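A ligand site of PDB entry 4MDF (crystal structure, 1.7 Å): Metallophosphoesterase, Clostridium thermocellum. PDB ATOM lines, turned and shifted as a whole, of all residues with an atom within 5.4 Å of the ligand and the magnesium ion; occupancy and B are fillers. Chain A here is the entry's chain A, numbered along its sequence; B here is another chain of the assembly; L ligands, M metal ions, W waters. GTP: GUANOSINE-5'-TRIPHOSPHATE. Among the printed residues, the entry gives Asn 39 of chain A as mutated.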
ATOM      1  N   GLY A  16     -28.162  -3.849  20.873  1.00  0.00           N
ATOM      2  CA  GLY A  16     -26.787  -3.961  21.318  1.00  0.00           C
ATOM      3  C   GLY A  16     -26.279  -5.382  21.277  1.00  0.00           C
ATOM      4  O   GLY A  16     -27.042  -6.324  21.418  1.00  0.00           O
ATOM      5  N   SER A  17     -24.975  -5.512  21.094  1.00  0.00           N
ATOM      6  CA  SER A  17     -24.283  -6.784  21.104  1.00  0.00           C
ATOM      7  C   SER A  17     -24.446  -7.506  22.431  1.00  0.00           C
ATOM      8  O   SER A  17     -24.721  -6.879  23.467  1.00  0.00           O
ATOM      9  CB  SER A  17     -22.793  -6.507  20.873  1.00  0.00           C
ATOM     10  OG  SER A  17     -22.022  -7.678  20.963  1.00  0.00           O
ATOM     11  N   SER A  18     -24.257  -8.818  22.433  1.00  0.00           N
ATOM     12  CA  SER A  18     -24.071  -9.491  23.698  1.00  0.00           C
ATOM     13  C   SER A  18     -22.914  -8.786  24.388  1.00  0.00           C
ATOM     14  O   SER A  18     -21.941  -8.385  23.734  1.00  0.00           O
ATOM     15  CB  SER A  18     -23.751 -10.968  23.483  1.00  0.00           C
ATOM     16  OG  SER A  18     -23.416 -11.592  24.715  1.00  0.00           O
ATOM     17  N   GLY A  19     -23.039  -8.575  25.699  1.00  0.00           N
ATOM     18  CA  GLY A  19     -21.984  -7.939  26.459  1.00  0.00           C
ATOM     19  C   GLY A  19     -22.048  -6.427  26.499  1.00  0.00           C
ATOM     20  O   GLY A  19     -21.235  -5.807  27.161  1.00  0.00           O
ATOM     21  N   SER A  20     -23.014  -5.827  25.791  1.00  0.00           N
ATOM     22  CA  SER A  20     -23.119  -4.374  25.742  1.00  0.00           C
ATOM     23  C   SER A  20     -23.802  -3.770  26.977  1.00  0.00           C
ATOM     24  O   SER A  20     -23.777  -2.560  27.169  1.00  0.00           O
ATOM     25  CB  SER A  20     -23.836  -3.895  24.463  1.00  0.00           C
ATOM     26  OG  SER A  20     -25.175  -4.374  24.428  1.00  0.00           O
ATOM     27  N   GLY A  21     -24.412  -4.623  27.791  1.00  0.00           N
ATOM     28  CA  GLY A  21     -25.011  -4.179  29.037  1.00  0.00           C
ATOM     29  C   GLY A  21     -26.504  -3.907  29.000  1.00  0.00           C
ATOM     30  O   GLY A  21     -27.026  -3.188  29.865  1.00  0.00           O
ATOM     31  N   LYS A  22     -27.183  -4.489  28.018  1.00  0.00           N
ATOM     32  CA  LYS A  22     -28.631  -4.306  27.870  1.00  0.00           C
ATOM     33  C   LYS A  22     -29.419  -4.678  29.118  1.00  0.00           C
ATOM     34  O   LYS A  22     -30.267  -3.912  29.589  1.00  0.00           O
ATOM     35  CB  LYS A  22     -29.155  -5.127  26.683  1.00  0.00           C
ATOM     36  CG  LYS A  22     -28.552  -4.729  25.336  1.00  0.00           C
ATOM     37  CD  LYS A  22     -29.145  -5.587  24.199  1.00  0.00           C
ATOM     38  CE  LYS A  22     -28.890  -7.090  24.397  1.00  0.00           C
ATOM     39  NZ  LYS A  22     -27.427  -7.363  24.330  1.00  0.00           N
ATOM     40  N   SER A  23     -29.177  -5.875  29.628  1.00  0.00           N
ATOM     41  CA  SER A  23     -29.971  -6.362  30.753  1.00  0.00           C
ATOM     42  C   SER A  23     -29.698  -5.553  32.008  1.00  0.00           C
ATOM     43  O   SER A  23     -30.613  -5.281  32.789  1.00  0.00           O
ATOM     44  CB  SER A  23     -29.740  -7.852  30.982  1.00  0.00           C
ATOM     45  OG  SER A  23     -30.118  -8.576  29.823  1.00  0.00           O
ATOM     46  N   THR A  24     -28.437  -5.175  32.204  1.00  0.00           N
ATOM     47  CA  THR A  24     -28.037  -4.354  33.350  1.00  0.00           C
ATOM     48  C   THR A  24     -28.743  -3.000  33.283  1.00  0.00           C
ATOM     49  O   THR A  24     -29.291  -2.516  34.274  1.00  0.00           O
ATOM     50  CB  THR A  24     -26.503  -4.153  33.380  1.00  0.00           C
ATOM     51  OG1 THR A  24     -25.880  -5.429  33.568  1.00  0.00           O
ATOM     52  CG2 THR A  24     -26.100  -3.233  34.506  1.00  0.00           C
ATOM     53  N   PHE A  25     -28.753  -2.425  32.080  1.00  0.00           N
ATOM     54  CA  PHE A  25     -29.402  -1.152  31.826  1.00  0.00           C
ATOM     55  C   PHE A  25     -30.901  -1.229  32.053  1.00  0.00           C
ATOM     56  O   PHE A  25     -31.502  -0.352  32.671  1.00  0.00           O
ATOM     57  CB  PHE A  25     -29.081  -0.742  30.376  1.00  0.00           C
ATOM     58  CG  PHE A  25     -29.734   0.540  29.912  1.00  0.00           C
ATOM     59  CD1 PHE A  25     -30.990   0.522  29.334  1.00  0.00           C
ATOM     60  CD2 PHE A  25     -29.045   1.741  29.993  1.00  0.00           C
ATOM     61  CE1 PHE A  25     -31.581   1.697  28.865  1.00  0.00           C
ATOM     62  CE2 PHE A  25     -29.624   2.925  29.525  1.00  0.00           C
ATOM     63  CZ  PHE A  25     -30.899   2.905  28.963  1.00  0.00           C
ATOM     64  N   ASN A  39     -33.724 -14.013  26.364  1.00  0.00           N
ATOM     65  CA  ASN A  39     -33.093 -15.086  27.124  1.00  0.00           C
ATOM     66  C   ASN A  39     -34.039 -15.647  28.186  1.00  0.00           C
ATOM     67  O   ASN A  39     -34.109 -16.862  28.386  1.00  0.00           O
ATOM     68  CB  ASN A  39     -31.757 -14.636  27.726  1.00  0.00           C
ATOM     69  CG  ASN A  39     -30.702 -14.370  26.652  1.00  0.00           C
ATOM     70  OD1 ASN A  39     -30.652 -15.065  25.644  1.00  0.00           O
ATOM     71  ND2 ASN A  39     -29.873 -13.347  26.864  1.00  0.00           N
ATOM     72  N   ASP A  79     -35.643  -6.602  25.748  1.00  0.00           N
ATOM     73  CA  ASP A  79     -34.254  -6.887  26.064  1.00  0.00           C
ATOM     74  C   ASP A  79     -33.807  -8.072  25.211  1.00  0.00           C
ATOM     75  O   ASP A  79     -33.918  -9.221  25.633  1.00  0.00           O
ATOM     76  CB  ASP A  79     -34.097  -7.178  27.564  1.00  0.00           C
ATOM     77  CG  ASP A  79     -32.663  -7.505  27.948  1.00  0.00           C
ATOM     78  OD1 ASP A  79     -31.744  -7.298  27.120  1.00  0.00           O
ATOM     79  OD2 ASP A  79     -32.446  -7.985  29.093  1.00  0.00           O
ATOM     80  N   THR A  81     -30.915  -8.623  21.474  1.00  0.00           N
ATOM     81  CA  THR A  81     -29.902  -7.846  20.755  1.00  0.00           C
ATOM     82  C   THR A  81     -30.515  -6.884  19.745  1.00  0.00           C
ATOM     83  O   THR A  81     -30.049  -5.754  19.606  1.00  0.00           O
ATOM     84  CB  THR A  81     -28.854  -8.726  20.067  1.00  0.00           C
ATOM     85  OG1 THR A  81     -29.497  -9.589  19.116  1.00  0.00           O
ATOM     86  CG2 THR A  81     -28.098  -9.555  21.117  1.00  0.00           C
ATOM     87  N   ARG A 117     -15.993  -7.342  28.664  1.00  0.00           N
ATOM     88  CA  ARG A 117     -17.075  -7.683  29.593  1.00  0.00           C
ATOM     89  C   ARG A 117     -17.476  -9.145  29.473  1.00  0.00           C
ATOM     90  O   ARG A 117     -17.670  -9.841  30.481  1.00  0.00           O
ATOM     91  CB  ARG A 117     -18.293  -6.793  29.338  1.00  0.00           C
ATOM     92  CG  ARG A 117     -18.055  -5.335  29.651  1.00  0.00           C
ATOM     93  CD  ARG A 117     -19.289  -4.523  29.371  1.00  0.00           C
ATOM     94  NE  ARG A 117     -19.127  -3.114  29.726  1.00  0.00           N
ATOM     95  CZ  ARG A 117     -20.058  -2.199  29.518  1.00  0.00           C
ATOM     96  NH1 ARG A 117     -21.202  -2.554  28.966  1.00  0.00           N
ATOM     97  NH2 ARG A 117     -19.840  -0.931  29.853  1.00  0.00           N
ATOM     98  N   ARG A 121     -17.532 -12.391  32.352  1.00  0.00           N
ATOM     99  CA  ARG A 121     -18.826 -12.878  32.829  1.00  0.00           C
ATOM    100  C   ARG A 121     -18.733 -14.243  33.480  1.00  0.00           C
ATOM    101  O   ARG A 121     -17.937 -15.078  33.068  1.00  0.00           O
ATOM    102  CB  ARG A 121     -19.831 -12.931  31.687  1.00  0.00           C
ATOM    103  CG  ARG A 121     -20.178 -11.575  31.112  1.00  0.00           C
ATOM    104  CD  ARG A 121     -21.225 -11.690  30.030  1.00  0.00           C
ATOM    105  NE  ARG A 121     -22.531 -12.074  30.570  1.00  0.00           N
ATOM    106  CZ  ARG A 121     -23.668 -11.972  29.888  1.00  0.00           C
ATOM    107  NH1 ARG A 121     -23.657 -11.494  28.648  1.00  0.00           N
ATOM    108  NH2 ARG A 121     -24.814 -12.360  30.440  1.00  0.00           N
ATOM    109  N   ASP A 123     -21.966 -15.613  34.453  1.00  0.00           N
ATOM    110  CA  ASP A 123     -23.325 -16.107  34.266  1.00  0.00           C
ATOM    111  C   ASP A 123     -23.497 -16.848  32.940  1.00  0.00           C
ATOM    112  O   ASP A 123     -24.088 -17.942  32.898  1.00  0.00           O
ATOM    113  CB  ASP A 123     -24.364 -14.993  34.423  1.00  0.00           C
ATOM    114  CG  ASP A 123     -24.142 -13.828  33.461  1.00  0.00           C
ATOM    115  OD1 ASP A 123     -22.990 -13.582  33.050  1.00  0.00           O
ATOM    116  OD2 ASP A 123     -25.141 -13.143  33.131  1.00  0.00           O
ATOM    117  N   ARG A 124     -22.976 -16.267  31.872  1.00  0.00           N
ATOM    118  CA  ARG A 124     -23.166 -16.782  30.517  1.00  0.00           C
ATOM    119  C   ARG A 124     -22.216 -16.021  29.617  1.00  0.00           C
ATOM    120  O   ARG A 124     -22.011 -14.823  29.800  1.00  0.00           O
ATOM    121  CB  ARG A 124     -24.612 -16.541  30.078  1.00  0.00           C
ATOM    122  CG  ARG A 124     -24.942 -17.013  28.672  1.00  0.00           C
ATOM    123  CD  ARG A 124     -26.448 -16.874  28.401  1.00  0.00           C
ATOM    124  NE  ARG A 124     -26.967 -15.609  28.912  1.00  0.00           N
ATOM    125  CZ  ARG A 124     -26.878 -14.442  28.269  1.00  0.00           C
ATOM    126  NH1 ARG A 124     -26.296 -14.387  27.075  1.00  0.00           N
ATOM    127  NH2 ARG A 124     -27.367 -13.341  28.814  1.00  0.00           N
ATOM    128  N   VAL A 126     -20.533 -15.731  25.328  1.00  0.00           N
ATOM    129  CA  VAL A 126     -20.570 -16.119  23.917  1.00  0.00           C
ATOM    130  C   VAL A 126     -19.148 -16.089  23.342  1.00  0.00           C
ATOM    131  O   VAL A 126     -18.233 -15.524  23.941  1.00  0.00           O
ATOM    132  CB  VAL A 126     -21.493 -15.215  23.077  1.00  0.00           C
ATOM    133  CG1 VAL A 126     -22.923 -15.262  23.620  1.00  0.00           C
ATOM    134  CG2 VAL A 126     -20.979 -13.783  23.039  1.00  0.00           C
ATOM    135  N   VAL A 162     -23.918   5.809  28.609  1.00  0.00           N
ATOM    136  CA  VAL A 162     -24.897   4.835  29.079  1.00  0.00           C
ATOM    137  C   VAL A 162     -25.205   5.060  30.557  1.00  0.00           C
ATOM    138  O   VAL A 162     -26.373   5.078  30.962  1.00  0.00           O
ATOM    139  CB  VAL A 162     -24.396   3.395  28.882  1.00  0.00           C
ATOM    140  CG1 VAL A 162     -25.335   2.401  29.581  1.00  0.00           C
ATOM    141  CG2 VAL A 162     -24.279   3.066  27.403  1.00  0.00           C
ATOM    142  O5'  DC B   1     -28.117 -12.404  24.846  1.00  0.00           O
ATOM    143  C5'  DC B   1     -27.207 -13.267  24.128  1.00  0.00           C
ATOM    144  C4'  DC B   1     -27.418 -13.025  22.644  1.00  0.00           C
ATOM    145  O4'  DC B   1     -26.388 -13.666  21.856  1.00  0.00           O
ATOM    146  C3'  DC B   1     -28.764 -13.549  22.154  1.00  0.00           C
ATOM    147  O3'  DC B   1     -29.312 -12.598  21.266  1.00  0.00           O
ATOM    148  C2'  DC B   1     -28.360 -14.813  21.412  1.00  0.00           C
ATOM    149  C1'  DC B   1     -27.041 -14.344  20.803  1.00  0.00           C
ATOM    150  N1   DC B   1     -26.210 -15.481  20.348  1.00  0.00           N
ATOM    151  C2   DC B   1     -25.839 -15.558  18.995  1.00  0.00           C
ATOM    152  O2   DC B   1     -26.189 -14.663  18.222  1.00  0.00           O
ATOM    153  N3   DC B   1     -25.083 -16.614  18.595  1.00  0.00           N
ATOM    154  C4   DC B   1     -24.743 -17.551  19.481  1.00  0.00           C
ATOM    155  N4   DC B   1     -24.001 -18.583  19.043  1.00  0.00           N
ATOM    156  C5   DC B   1     -25.112 -17.491  20.852  1.00  0.00           C
ATOM    157  C6   DC B   1     -25.851 -16.441  21.239  1.00  0.00           C
HETATM  158  PG  GTP L   1     -26.475 -10.498  26.589  1.00  0.00           P
HETATM  159  O1G GTP L   1     -25.446 -11.590  26.432  1.00  0.00           O
HETATM  160  O2G GTP L   1     -27.020 -10.112  25.233  1.00  0.00           O
HETATM  161  O3G GTP L   1     -27.593 -10.939  27.514  1.00  0.00           O
HETATM  162  O3B GTP L   1     -25.606  -9.296  27.226  1.00  0.00           O
HETATM  163  PB  GTP L   1     -26.225  -7.939  27.822  1.00  0.00           P
HETATM  164  O1B GTP L   1     -27.572  -8.167  28.450  1.00  0.00           O
HETATM  165  O2B GTP L   1     -26.238  -6.871  26.735  1.00  0.00           O
HETATM  166  O3A GTP L   1     -25.127  -7.497  28.906  1.00  0.00           O
HETATM  167  PA  GTP L   1     -25.268  -7.594  30.508  1.00  0.00           P
HETATM  168  O1A GTP L   1     -25.625  -8.993  30.933  1.00  0.00           O
HETATM  169  O2A GTP L   1     -26.216  -6.568  31.064  1.00  0.00           O
HETATM  170  O5' GTP L   1     -23.759  -7.268  30.952  1.00  0.00           O
HETATM  171  C5' GTP L   1     -22.667  -8.041  30.498  1.00  0.00           C
HETATM  172  C4' GTP L   1     -21.551  -7.889  31.528  1.00  0.00           C
HETATM  173  O4' GTP L   1     -21.091  -6.556  31.478  1.00  0.00           O
HETATM  174  C3' GTP L   1     -22.084  -8.137  32.934  1.00  0.00           C
HETATM  175  O3' GTP L   1     -21.138  -8.891  33.642  1.00  0.00           O
HETATM  176  C2' GTP L   1     -22.190  -6.763  33.539  1.00  0.00           C
HETATM  177  O2' GTP L   1     -21.982  -6.786  34.935  1.00  0.00           O
HETATM  178  C1' GTP L   1     -21.176  -5.942  32.749  1.00  0.00           C
HETATM  179  N9  GTP L   1     -21.741  -4.601  32.610  1.00  0.00           N
HETATM  180  C8  GTP L   1     -23.012  -4.325  32.177  1.00  0.00           C
HETATM  181  N7  GTP L   1     -23.185  -2.980  32.192  1.00  0.00           N
HETATM  182  C5  GTP L   1     -22.041  -2.404  32.624  1.00  0.00           C
HETATM  183  C6  GTP L   1     -21.681  -1.083  32.820  1.00  0.00           C
HETATM  184  O6  GTP L   1     -22.503  -0.193  32.587  1.00  0.00           O
HETATM  185  N1  GTP L   1     -20.420  -0.773  33.277  1.00  0.00           N
HETATM  186  C2  GTP L   1     -19.521  -1.793  33.542  1.00  0.00           C
HETATM  187  N2  GTP L   1     -18.302  -1.510  33.991  1.00  0.00           N
HETATM  188  N3  GTP L   1     -19.890  -3.114  33.342  1.00  0.00           N
HETATM  189  C4  GTP L   1     -21.131  -3.416  32.890  1.00  0.00           C
HETATM  190 MG    MG M   1     -28.866  -9.758  28.641  1.00  0.00          MG
HETATM  191  O   HOH W   1     -27.767 -10.365  30.401  1.00  0.00           O
HETATM  192  O   HOH W   2     -19.631  -7.354  36.204  1.00  0.00           O
HETATM  193  O   HOH W   3     -18.326  -8.733  32.844  1.00  0.00           O
HETATM  194  O   HOH W   4     -25.509  -1.205  31.062  1.00  0.00           O
HETATM  195  O   HOH W   5     -30.220 -11.359  28.992  1.00  0.00           O
HETATM  196  O   HOH W   6     -30.048  -9.180  26.993  1.00  0.00           O
HETATM  197  O   HOH W   7     -25.130 -10.220  33.203  1.00  0.00           O
HETATM  198  O   HOH W   8     -21.888   2.300  31.673  1.00  0.00           O
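An oxygen (O2A) of the ligand lies within hydrogen-bond range of the backbone NH of Ser 23, at 3.4 Å. O5' of DC 1 of chain B sits close to an oxygen (O2G) of the ligand (2.6 Å). OG of Ser 18 is in hydrogen-bond range of O1G of the ligand, 2.7 Å away. The backbone NH of Lys 22 sits at hydrogen-bond distance from an oxygen (O2B) of the ligand (2.9 Å). NZ of Lys 22 is in salt-bridge range of O2B of the ligand, 2.7 Å away. The guanidinium group of Arg 124 is in salt-bridge range of an oxygen (O1G) of the ligand (3.0 Å). The backbone NH (N) of Thr 24 is in hydrogen-bond range of an oxygen (O2A) of the ligand, 2.9 Å away. O2A of the ligand is in hydrogen-bond range of OG1 of Thr 24. O1G of the ligand is in salt-bridge range of NH1 of Arg 121, 2.8 Å away. The backbone NH (N) of Gly 19 is in hydrogen-bond range of an oxygen (O3B) of the ligand. An oxygen (O2B) of the ligand lies within hydrogen-bond range of the backbone NH (N) of Gly 21, 3.1 Å away. The side-chain amide nitrogen (ND2) of Asn 39 lies close to an oxygen (O3G) of the ligand (3.4 Å).
The side-chain carboxylate (OD2) of Asp 79 sits close to the side-chain hydroxyl (OG) of Ser 23. O5' of DC 1 of chain B sits close to NH1 of Arg 124, 3.5 Å away. O5' of DC 1 of chain B is in hydrogen-bond range of ND2 of Asn 39 (2.8 Å). The side-chain amino group (NZ) of Lys 22 is in hydrogen-bond range of the backbone carbonyl oxygen (O) of Ser 17 (2.9 Å). The side-chain amino group (NZ) of Lys 22 sits at hydrogen-bond distance from the backbone carbonyl oxygen (O) of Gly 16, 3.1 Å away. The guanidinium group (NH2) of Arg 124 lies close to the side-chain amide nitrogen (ND2) of Asn 39, at 3.2 Å. The guanidinium group of Arg 117 sits at hydrogen-bond distance from the backbone carbonyl oxygen of Ser 20, 3.1 Å away. OG of Ser 20 is in hydrogen-bond range of O of Ser 17, 2.7 Å away.
N1 of the ligand lies close to NH2 of Arg 117 (3.5 Å). Ser 17 touches the ligand (O to O2B, 3.6 Å). N of Ser 20 touches O2B of the ligand, at 3.5 Å.
Merely in contact with the magnesium ion: Arg 124 (3.9 Å). The nearest printed residue that does not touch the magnesium ion is Asp 79 (4.02 Å).
The magnesium ion is bound by O1B of the ligand, O3G of the ligand, OG of Ser 23, water W6, water W5 and water W1.
Water W5 lies within hydrogen-bond range of the side-chain amide nitrogen of Asn 39 and the guanidinium group of Arg 124. Water W1 bridges an oxygen (O1A) of the ligand (2.6 Å) and the guanidinium group (NH2) of Arg 124 (3.4 Å). Water W7 lies within hydrogen-bond range of an oxygen (O1A) of the ligand (2.6 Å) and the side-chain carboxylate of Asp 123 (2.9 Å). Water W3 lies within hydrogen-bond range of O of Arg 117 (2.7 Å) and O3' of the ligand (2.9 Å). Water W4 lies within hydrogen-bond range of the backbone carbonyl oxygen (O) of Gly 21 (2.8 Å) and a nitrogen (N7) of the ligand (3.1 Å).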
